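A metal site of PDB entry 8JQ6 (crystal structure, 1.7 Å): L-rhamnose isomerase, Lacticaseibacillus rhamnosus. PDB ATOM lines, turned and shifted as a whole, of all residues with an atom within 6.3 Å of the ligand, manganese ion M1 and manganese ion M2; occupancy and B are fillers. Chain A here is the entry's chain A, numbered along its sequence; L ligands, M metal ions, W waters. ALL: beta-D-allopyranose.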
ATOM      1  N   TRP A  42      -7.055   2.068   6.674  1.00  0.00           N
ATOM      2  CA  TRP A  42      -7.274   2.971   7.843  1.00  0.00           C
ATOM      3  C   TRP A  42      -7.292   2.191   9.164  1.00  0.00           C
ATOM      4  O   TRP A  42      -7.169   2.833  10.228  1.00  0.00           O
ATOM      5  CB  TRP A  42      -8.534   3.833   7.670  1.00  0.00           C
ATOM      6  CG  TRP A  42      -9.799   3.138   7.267  1.00  0.00           C
ATOM      7  CD1 TRP A  42     -10.786   2.687   8.098  1.00  0.00           C
ATOM      8  CD2 TRP A  42     -10.265   2.908   5.930  1.00  0.00           C
ATOM      9  NE1 TRP A  42     -11.830   2.183   7.368  1.00  0.00           N
ATOM     10  CE2 TRP A  42     -11.527   2.291   6.037  1.00  0.00           C
ATOM     11  CE3 TRP A  42      -9.729   3.141   4.657  1.00  0.00           C
ATOM     12  CZ2 TRP A  42     -12.251   1.906   4.916  1.00  0.00           C
ATOM     13  CZ3 TRP A  42     -10.449   2.772   3.553  1.00  0.00           C
ATOM     14  CH2 TRP A  42     -11.697   2.150   3.678  1.00  0.00           C
ATOM     15  N   ILE A  47      -7.453   5.523  11.404  1.00  0.00           N
ATOM     16  CA  ILE A  47      -8.036   6.499  10.436  1.00  0.00           C
ATOM     17  C   ILE A  47      -7.418   7.900  10.613  1.00  0.00           C
ATOM     18  O   ILE A  47      -8.094   8.876  10.252  1.00  0.00           O
ATOM     19  CB  ILE A  47      -9.569   6.544  10.557  1.00  0.00           C
ATOM     20  CG1 ILE A  47     -10.130   5.199  11.050  1.00  0.00           C
ATOM     21  CG2 ILE A  47     -10.185   6.993   9.240  1.00  0.00           C
ATOM     22  CD1 ILE A  47     -11.635   5.140  11.116  1.00  0.00           C
ATOM     23  N   HIS A  97      -7.871   6.022   1.613  1.00  0.00           N
ATOM     24  CA  HIS A  97      -8.681   7.221   1.906  1.00  0.00           C
ATOM     25  C   HIS A  97      -7.916   8.452   1.429  1.00  0.00           C
ATOM     26  O   HIS A  97      -6.680   8.403   1.379  1.00  0.00           O
ATOM     27  CB  HIS A  97      -9.035   7.311   3.388  1.00  0.00           C
ATOM     28  CG  HIS A  97     -10.507   7.233   3.641  1.00  0.00           C
ATOM     29  ND1 HIS A  97     -11.352   8.292   3.365  1.00  0.00           N
ATOM     30  CD2 HIS A  97     -11.269   6.251   4.147  1.00  0.00           C
ATOM     31  CE1 HIS A  97     -12.583   7.945   3.676  1.00  0.00           C
ATOM     32  NE2 HIS A  97     -12.560   6.696   4.163  1.00  0.00           N
ATOM     33  N   ASN A 134     -11.408   5.973  -1.502  1.00  0.00           N
ATOM     34  CA  ASN A 134     -12.514   6.626  -0.746  1.00  0.00           C
ATOM     35  C   ASN A 134     -12.170   8.101  -0.579  1.00  0.00           C
ATOM     36  O   ASN A 134     -11.100   8.417  -0.013  1.00  0.00           O
ATOM     37  CB  ASN A 134     -12.712   6.016   0.648  1.00  0.00           C
ATOM     38  CG  ASN A 134     -13.042   4.539   0.624  1.00  0.00           C
ATOM     39  OD1 ASN A 134     -14.198   4.156   0.811  1.00  0.00           O
ATOM     40  ND2 ASN A 134     -12.039   3.708   0.379  1.00  0.00           N
ATOM     41  N   GLY A 135     -13.046   8.975  -1.062  1.00  0.00           N
ATOM     42  CA  GLY A 135     -13.048  10.391  -0.671  1.00  0.00           C
ATOM     43  C   GLY A 135     -13.278  10.494   0.826  1.00  0.00           C
ATOM     44  O   GLY A 135     -14.010   9.633   1.373  1.00  0.00           O
ATOM     45  N   PHE A 138     -15.293  13.622   6.181  1.00  0.00           N
ATOM     46  CA  PHE A 138     -15.453  13.651   7.662  1.00  0.00           C
ATOM     47  C   PHE A 138     -14.163  14.154   8.318  1.00  0.00           C
ATOM     48  O   PHE A 138     -13.128  14.286   7.616  1.00  0.00           O
ATOM     49  CB  PHE A 138     -15.872  12.273   8.177  1.00  0.00           C
ATOM     50  CG  PHE A 138     -14.913  11.160   7.850  1.00  0.00           C
ATOM     51  CD1 PHE A 138     -13.801  10.923   8.637  1.00  0.00           C
ATOM     52  CD2 PHE A 138     -15.127  10.331   6.760  1.00  0.00           C
ATOM     53  CE1 PHE A 138     -12.925   9.888   8.331  1.00  0.00           C
ATOM     54  CE2 PHE A 138     -14.261   9.296   6.467  1.00  0.00           C
ATOM     55  CZ  PHE A 138     -13.146   9.080   7.241  1.00  0.00           C
ATOM     56  N   ASN A 185     -15.266   4.927  -3.815  1.00  0.00           N
ATOM     57  CA  ASN A 185     -16.434   4.788  -2.909  1.00  0.00           C
ATOM     58  C   ASN A 185     -16.733   6.129  -2.234  1.00  0.00           C
ATOM     59  O   ASN A 185     -15.806   6.711  -1.635  1.00  0.00           O
ATOM     60  CB  ASN A 185     -16.222   3.695  -1.865  1.00  0.00           C
ATOM     61  CG  ASN A 185     -17.433   3.502  -0.977  1.00  0.00           C
ATOM     62  OD1 ASN A 185     -18.499   3.152  -1.458  1.00  0.00           O
ATOM     63  ND2 ASN A 185     -17.268   3.705   0.319  1.00  0.00           N
ATOM     64  N   TRP A 187     -18.818   7.831   0.719  1.00  0.00           N
ATOM     65  CA  TRP A 187     -19.615   7.806   1.966  1.00  0.00           C
ATOM     66  C   TRP A 187     -19.684   9.212   2.546  1.00  0.00           C
ATOM     67  O   TRP A 187     -18.635   9.839   2.713  1.00  0.00           O
ATOM     68  CB  TRP A 187     -19.084   6.800   2.997  1.00  0.00           C
ATOM     69  CG  TRP A 187     -19.900   6.911   4.246  1.00  0.00           C
ATOM     70  CD1 TRP A 187     -21.192   6.492   4.409  1.00  0.00           C
ATOM     71  CD2 TRP A 187     -19.558   7.633   5.439  1.00  0.00           C
ATOM     72  NE1 TRP A 187     -21.666   6.886   5.634  1.00  0.00           N
ATOM     73  CE2 TRP A 187     -20.668   7.565   6.299  1.00  0.00           C
ATOM     74  CE3 TRP A 187     -18.409   8.297   5.885  1.00  0.00           C
ATOM     75  CZ2 TRP A 187     -20.670   8.127   7.576  1.00  0.00           C
ATOM     76  CZ3 TRP A 187     -18.395   8.845   7.152  1.00  0.00           C
ATOM     77  CH2 TRP A 187     -19.514   8.770   7.977  1.00  0.00           C
ATOM     78  N   GLU A 228     -22.293   4.650  -0.940  1.00  0.00           N
ATOM     79  CA  GLU A 228     -22.458   3.888   0.318  1.00  0.00           C
ATOM     80  C   GLU A 228     -23.474   4.591   1.215  1.00  0.00           C
ATOM     81  O   GLU A 228     -23.169   5.680   1.724  1.00  0.00           O
ATOM     82  CB  GLU A 228     -21.113   3.764   1.033  1.00  0.00           C
ATOM     83  CG  GLU A 228     -21.231   3.081   2.375  1.00  0.00           C
ATOM     84  CD  GLU A 228     -19.907   2.787   3.058  1.00  0.00           C
ATOM     85  OE1 GLU A 228     -18.866   3.286   2.589  1.00  0.00           O
ATOM     86  OE2 GLU A 228     -19.928   2.052   4.040  1.00  0.00           O
ATOM     87  N   LYS A 230     -26.157   4.511   4.707  1.00  0.00           N
ATOM     88  CA  LYS A 230     -26.073   4.175   6.142  1.00  0.00           C
ATOM     89  C   LYS A 230     -27.460   4.399   6.726  1.00  0.00           C
ATOM     90  O   LYS A 230     -28.171   5.260   6.203  1.00  0.00           O
ATOM     91  CB  LYS A 230     -25.009   5.075   6.776  1.00  0.00           C
ATOM     92  CG  LYS A 230     -24.534   4.662   8.151  1.00  0.00           C
ATOM     93  CD  LYS A 230     -23.291   5.415   8.565  1.00  0.00           C
ATOM     94  CE  LYS A 230     -22.689   4.918   9.850  1.00  0.00           C
ATOM     95  NZ  LYS A 230     -21.442   5.655  10.165  1.00  0.00           N
ATOM     96  N   THR A 259     -22.804   0.509  -2.903  1.00  0.00           N
ATOM     97  CA  THR A 259     -22.002  -0.047  -1.788  1.00  0.00           C
ATOM     98  C   THR A 259     -22.930  -0.525  -0.677  1.00  0.00           C
ATOM     99  O   THR A 259     -23.680   0.304  -0.135  1.00  0.00           O
ATOM    100  CB  THR A 259     -20.975   0.946  -1.237  1.00  0.00           C
ATOM    101  OG1 THR A 259     -20.055   1.252  -2.282  1.00  0.00           O
ATOM    102  CG2 THR A 259     -20.235   0.388  -0.032  1.00  0.00           C
ATOM    103  N   ASP A 261     -22.670  -1.959   2.992  1.00  0.00           N
ATOM    104  CA  ASP A 261     -21.837  -2.195   4.198  1.00  0.00           C
ATOM    105  C   ASP A 261     -22.684  -2.980   5.201  1.00  0.00           C
ATOM    106  O   ASP A 261     -23.748  -2.491   5.587  1.00  0.00           O
ATOM    107  CB  ASP A 261     -21.272  -0.884   4.761  1.00  0.00           C
ATOM    108  CG  ASP A 261     -20.413  -1.106   5.979  1.00  0.00           C
ATOM    109  OD1 ASP A 261     -19.293  -0.559   6.014  1.00  0.00           O
ATOM    110  OD2 ASP A 261     -20.859  -1.823   6.888  1.00  0.00           O
ATOM    111  N   GLY A 263     -22.651  -3.543   8.151  1.00  0.00           N
ATOM    112  CA  GLY A 263     -22.851  -2.963   9.500  1.00  0.00           C
ATOM    113  C   GLY A 263     -23.897  -1.862   9.535  1.00  0.00           C
ATOM    114  O   GLY A 263     -24.202  -1.358  10.630  1.00  0.00           O
ATOM    115  N   HIS A 264     -24.473  -1.482   8.390  1.00  0.00           N
ATOM    116  CA  HIS A 264     -25.184  -0.175   8.252  1.00  0.00           C
ATOM    117  C   HIS A 264     -26.696  -0.370   8.084  1.00  0.00           C
ATOM    118  O   HIS A 264     -27.354   0.610   7.664  1.00  0.00           O
ATOM    119  CB  HIS A 264     -24.598   0.610   7.078  1.00  0.00           C
ATOM    120  CG  HIS A 264     -23.199   1.081   7.301  1.00  0.00           C
ATOM    121  ND1 HIS A 264     -22.591   1.969   6.453  1.00  0.00           N
ATOM    122  CD2 HIS A 264     -22.310   0.824   8.281  1.00  0.00           C
ATOM    123  CE1 HIS A 264     -21.370   2.215   6.875  1.00  0.00           C
ATOM    124  NE2 HIS A 264     -21.174   1.535   8.009  1.00  0.00           N
ATOM    125  N   HIS A 288     -19.033  -4.207   1.388  1.00  0.00           N
ATOM    126  CA  HIS A 288     -18.180  -3.904   2.568  1.00  0.00           C
ATOM    127  C   HIS A 288     -18.544  -4.853   3.709  1.00  0.00           C
ATOM    128  O   HIS A 288     -19.567  -4.598   4.369  1.00  0.00           O
ATOM    129  CB  HIS A 288     -18.350  -2.463   3.062  1.00  0.00           C
ATOM    130  CG  HIS A 288     -17.524  -1.467   2.334  1.00  0.00           C
ATOM    131  ND1 HIS A 288     -17.345  -0.185   2.826  1.00  0.00           N
ATOM    132  CD2 HIS A 288     -16.848  -1.542   1.166  1.00  0.00           C
ATOM    133  CE1 HIS A 288     -16.572   0.492   1.990  1.00  0.00           C
ATOM    134  NE2 HIS A 288     -16.269  -0.315   0.962  1.00  0.00           N
ATOM    135  N   SER A 290     -18.259  -6.101   7.361  1.00  0.00           N
ATOM    136  CA  SER A 290     -18.079  -5.370   8.626  1.00  0.00           C
ATOM    137  C   SER A 290     -19.003  -6.035   9.645  1.00  0.00           C
ATOM    138  O   SER A 290     -20.077  -6.471   9.226  1.00  0.00           O
ATOM    139  CB  SER A 290     -18.421  -3.912   8.440  1.00  0.00           C
ATOM    140  OG  SER A 290     -18.026  -3.165   9.578  1.00  0.00           O
ATOM    141  N   ASP A 296     -23.506   0.359  14.388  1.00  0.00           N
ATOM    142  CA  ASP A 296     -22.407   0.392  13.389  1.00  0.00           C
ATOM    143  C   ASP A 296     -21.070   0.519  14.125  1.00  0.00           C
ATOM    144  O   ASP A 296     -20.467   1.608  14.075  1.00  0.00           O
ATOM    145  CB  ASP A 296     -22.577   1.548  12.412  1.00  0.00           C
ATOM    146  CG  ASP A 296     -21.460   1.588  11.390  1.00  0.00           C
ATOM    147  OD1 ASP A 296     -20.960   0.498  11.043  1.00  0.00           O
ATOM    148  OD2 ASP A 296     -21.089   2.703  10.971  1.00  0.00           O
ATOM    149  N   SER A 297     -20.630  -0.580  14.746  1.00  0.00           N
ATOM    150  CA  SER A 297     -19.502  -0.623  15.714  1.00  0.00           C
ATOM    151  C   SER A 297     -18.170  -0.934  15.009  1.00  0.00           C
ATOM    152  O   SER A 297     -17.113  -0.753  15.636  1.00  0.00           O
ATOM    153  CB  SER A 297     -19.772  -1.627  16.798  1.00  0.00           C
ATOM    154  OG  SER A 297     -20.038  -2.907  16.246  1.00  0.00           O
ATOM    155  N   ASP A 298     -18.234  -1.406  13.767  1.00  0.00           N
ATOM    156  CA  ASP A 298     -17.034  -1.658  12.936  1.00  0.00           C
ATOM    157  C   ASP A 298     -16.116  -2.688  13.617  1.00  0.00           C
ATOM    158  O   ASP A 298     -14.881  -2.536  13.551  1.00  0.00           O
ATOM    159  CB  ASP A 298     -16.347  -0.326  12.614  1.00  0.00           C
ATOM    160  CG  ASP A 298     -17.224   0.527  11.716  1.00  0.00           C
ATOM    161  OD1 ASP A 298     -17.952  -0.056  10.905  1.00  0.00           O
ATOM    162  OD2 ASP A 298     -17.206   1.760  11.844  1.00  0.00           O
ATOM    163  N   ASP A 328     -14.244  -3.488   5.847  1.00  0.00           N
ATOM    164  CA  ASP A 328     -14.397  -2.193   6.549  1.00  0.00           C
ATOM    165  C   ASP A 328     -14.648  -2.461   8.029  1.00  0.00           C
ATOM    166  O   ASP A 328     -15.743  -2.906   8.411  1.00  0.00           O
ATOM    167  CB  ASP A 328     -15.487  -1.325   5.938  1.00  0.00           C
ATOM    168  CG  ASP A 328     -15.438   0.103   6.470  1.00  0.00           C
ATOM    169  OD1 ASP A 328     -16.281   0.897   6.067  1.00  0.00           O
ATOM    170  OD2 ASP A 328     -14.546   0.394   7.287  1.00  0.00           O
HETATM  171  C1  ALL L   1     -17.246   4.989   8.680  1.00  0.00           C
HETATM  172  C2  ALL L   1     -18.532   5.032   7.846  1.00  0.00           C
HETATM  173  C3  ALL L   1     -18.471   4.119   6.613  1.00  0.00           C
HETATM  174  C4  ALL L   1     -17.161   4.342   5.821  1.00  0.00           C
HETATM  175  C5  ALL L   1     -15.949   4.274   6.782  1.00  0.00           C
HETATM  176  C6  ALL L   1     -14.632   4.570   6.079  1.00  0.00           C
HETATM  177  O1  ALL L   1     -17.296   6.030   9.689  1.00  0.00           O
HETATM  178  O2  ALL L   1     -19.632   4.624   8.653  1.00  0.00           O
HETATM  179  O3  ALL L   1     -18.588   2.760   7.077  1.00  0.00           O
HETATM  180  O4  ALL L   1     -17.017   3.415   4.711  1.00  0.00           O
HETATM  181  O5  ALL L   1     -16.097   5.210   7.851  1.00  0.00           O
HETATM  182  O6  ALL L   1     -14.827   5.503   5.011  1.00  0.00           O
HETATM  183 MN    MN M   1     -18.193   1.017   4.856  1.00  0.00          MN
HETATM  184 MN    MN M   2     -19.564   0.828   9.686  1.00  0.00          MN
HETATM  185  O   HOH W   1     -19.003   2.712   9.713  1.00  0.00           O
HETATM  186  O   HOH W   2     -19.904  -1.414   9.216  1.00  0.00           O
HETATM  187  O   HOH W   3     -15.853   5.742   2.379  1.00  0.00           O
HETATM  188  O   HOH W   4     -18.193   0.506   8.188  1.00  0.00           O
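A ring nitrogen (NE2) of His 264 sits close to an oxygen (O3) of the ligand, 3.0 Å away.
The side-chain carboxylate (OD2) of Asp 296 lies within hydrogen-bond range of an oxygen (O2) of the ligand (3.3 Å).
An oxygen (O2) of the ligand is in hydrogen-bond range of the side-chain amino group of Lys 230 (2.6 Å).
NE2 of His 97 lies within hydrogen-bond range of O6 of the ligand (2.7 Å).
N of Ile 47 lies within hydrogen-bond range of O of Trp 42, 2.9 Å away.
The side-chain hydroxyl (OG) of Ser 290 is in hydrogen-bond range of the backbone carbonyl oxygen (O) of Asp 328 (2.6 Å).
The side-chain carboxylate (OD1) of Asp 298 lies close to the side-chain hydroxyl (OG) of Ser 290, at 3.4 Å.
The backbone carbonyl oxygen of Asn 134 lies close to a ring nitrogen (ND1) of His 97, 3.4 Å away.
The backbone NH (N) of Gly 263 lies within hydrogen-bond range of the side-chain carboxylate (OD2) of Asp 261 (2.8 Å).
The side-chain carboxylate of Glu 228 sits at hydrogen-bond distance from the side-chain amide nitrogen of Asn 185 (2.8 Å).
OD2 of Asp 296 lies within salt-bridge range of NZ of Lys 230 (3.1 Å).
OD2 of Asp 328 lies within hydrogen-bond range of NE1 of Trp 42 (3.3 Å).
Merely in contact with the ligand: Trp 42 (3.8 Å) and Trp 187 (3.7 Å).
Hydrophobic or aromatic side chains within 4 Å of the ligand: Trp 42, His 97, Trp 187 and His 264.
Nine residues have an atom within 4 Å of the ligand: Trp 42, His 97, Trp 187, Glu 228, Lys 230, Asp 261, His 264, Asp 296 and Asp 328.
Four residues have an atom within 4 Å of manganese ion M2: Asp 261, His 264, Asp 296 and Asp 298.
The nearest printed residue that does not touch manganese ion M2 is Ser 290 (4.3 Å).
Manganese ion M1 is bound by OE2 of Glu 228 (2.2 Å), OD1 of Asp 261 (2.2 Å), OD1 of Asp 328 (2.3 Å), ND1 of His 288 (2.5 Å) and O4 of the ligand (2.7 Å).
Slightly farther from manganese ion M1 lies an oxygen (O3) of the ligand (2.9 Å).
Manganese ion M2 is bound by water W1 (2.0 Å), the side-chain carboxylate (OD1) of Asp 296 (2.0 Å), water W4 (2.1 Å), the side-chain carboxylate (OD1) of Asp 298 (2.2 Å), water W2 (2.3 Å) and a ring nitrogen (NE2) of His 264 (2.4 Å).
Slightly farther from manganese ion M2 lies OD2 of Asp 296 (2.7 Å).
Water W2 bridges the side-chain carboxylate of Asp 261 (2.5 Å) and the side-chain hydroxyl of Ser 290 (2.6 Å).
Water W1 lies within hydrogen-bond range of the side-chain carboxylate (OD2) of Asp 296 (2.4 Å), an oxygen (O3) of the ligand (2.7 Å) and the side-chain carboxylate (OD2) of Asp 298 (2.9 Å).
Water W3 lies within hydrogen-bond range of OD1 of Asn 134 (2.8 Å), O6 of the ligand (2.8 Å) and ND2 of Asn 185 (3.2 Å).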
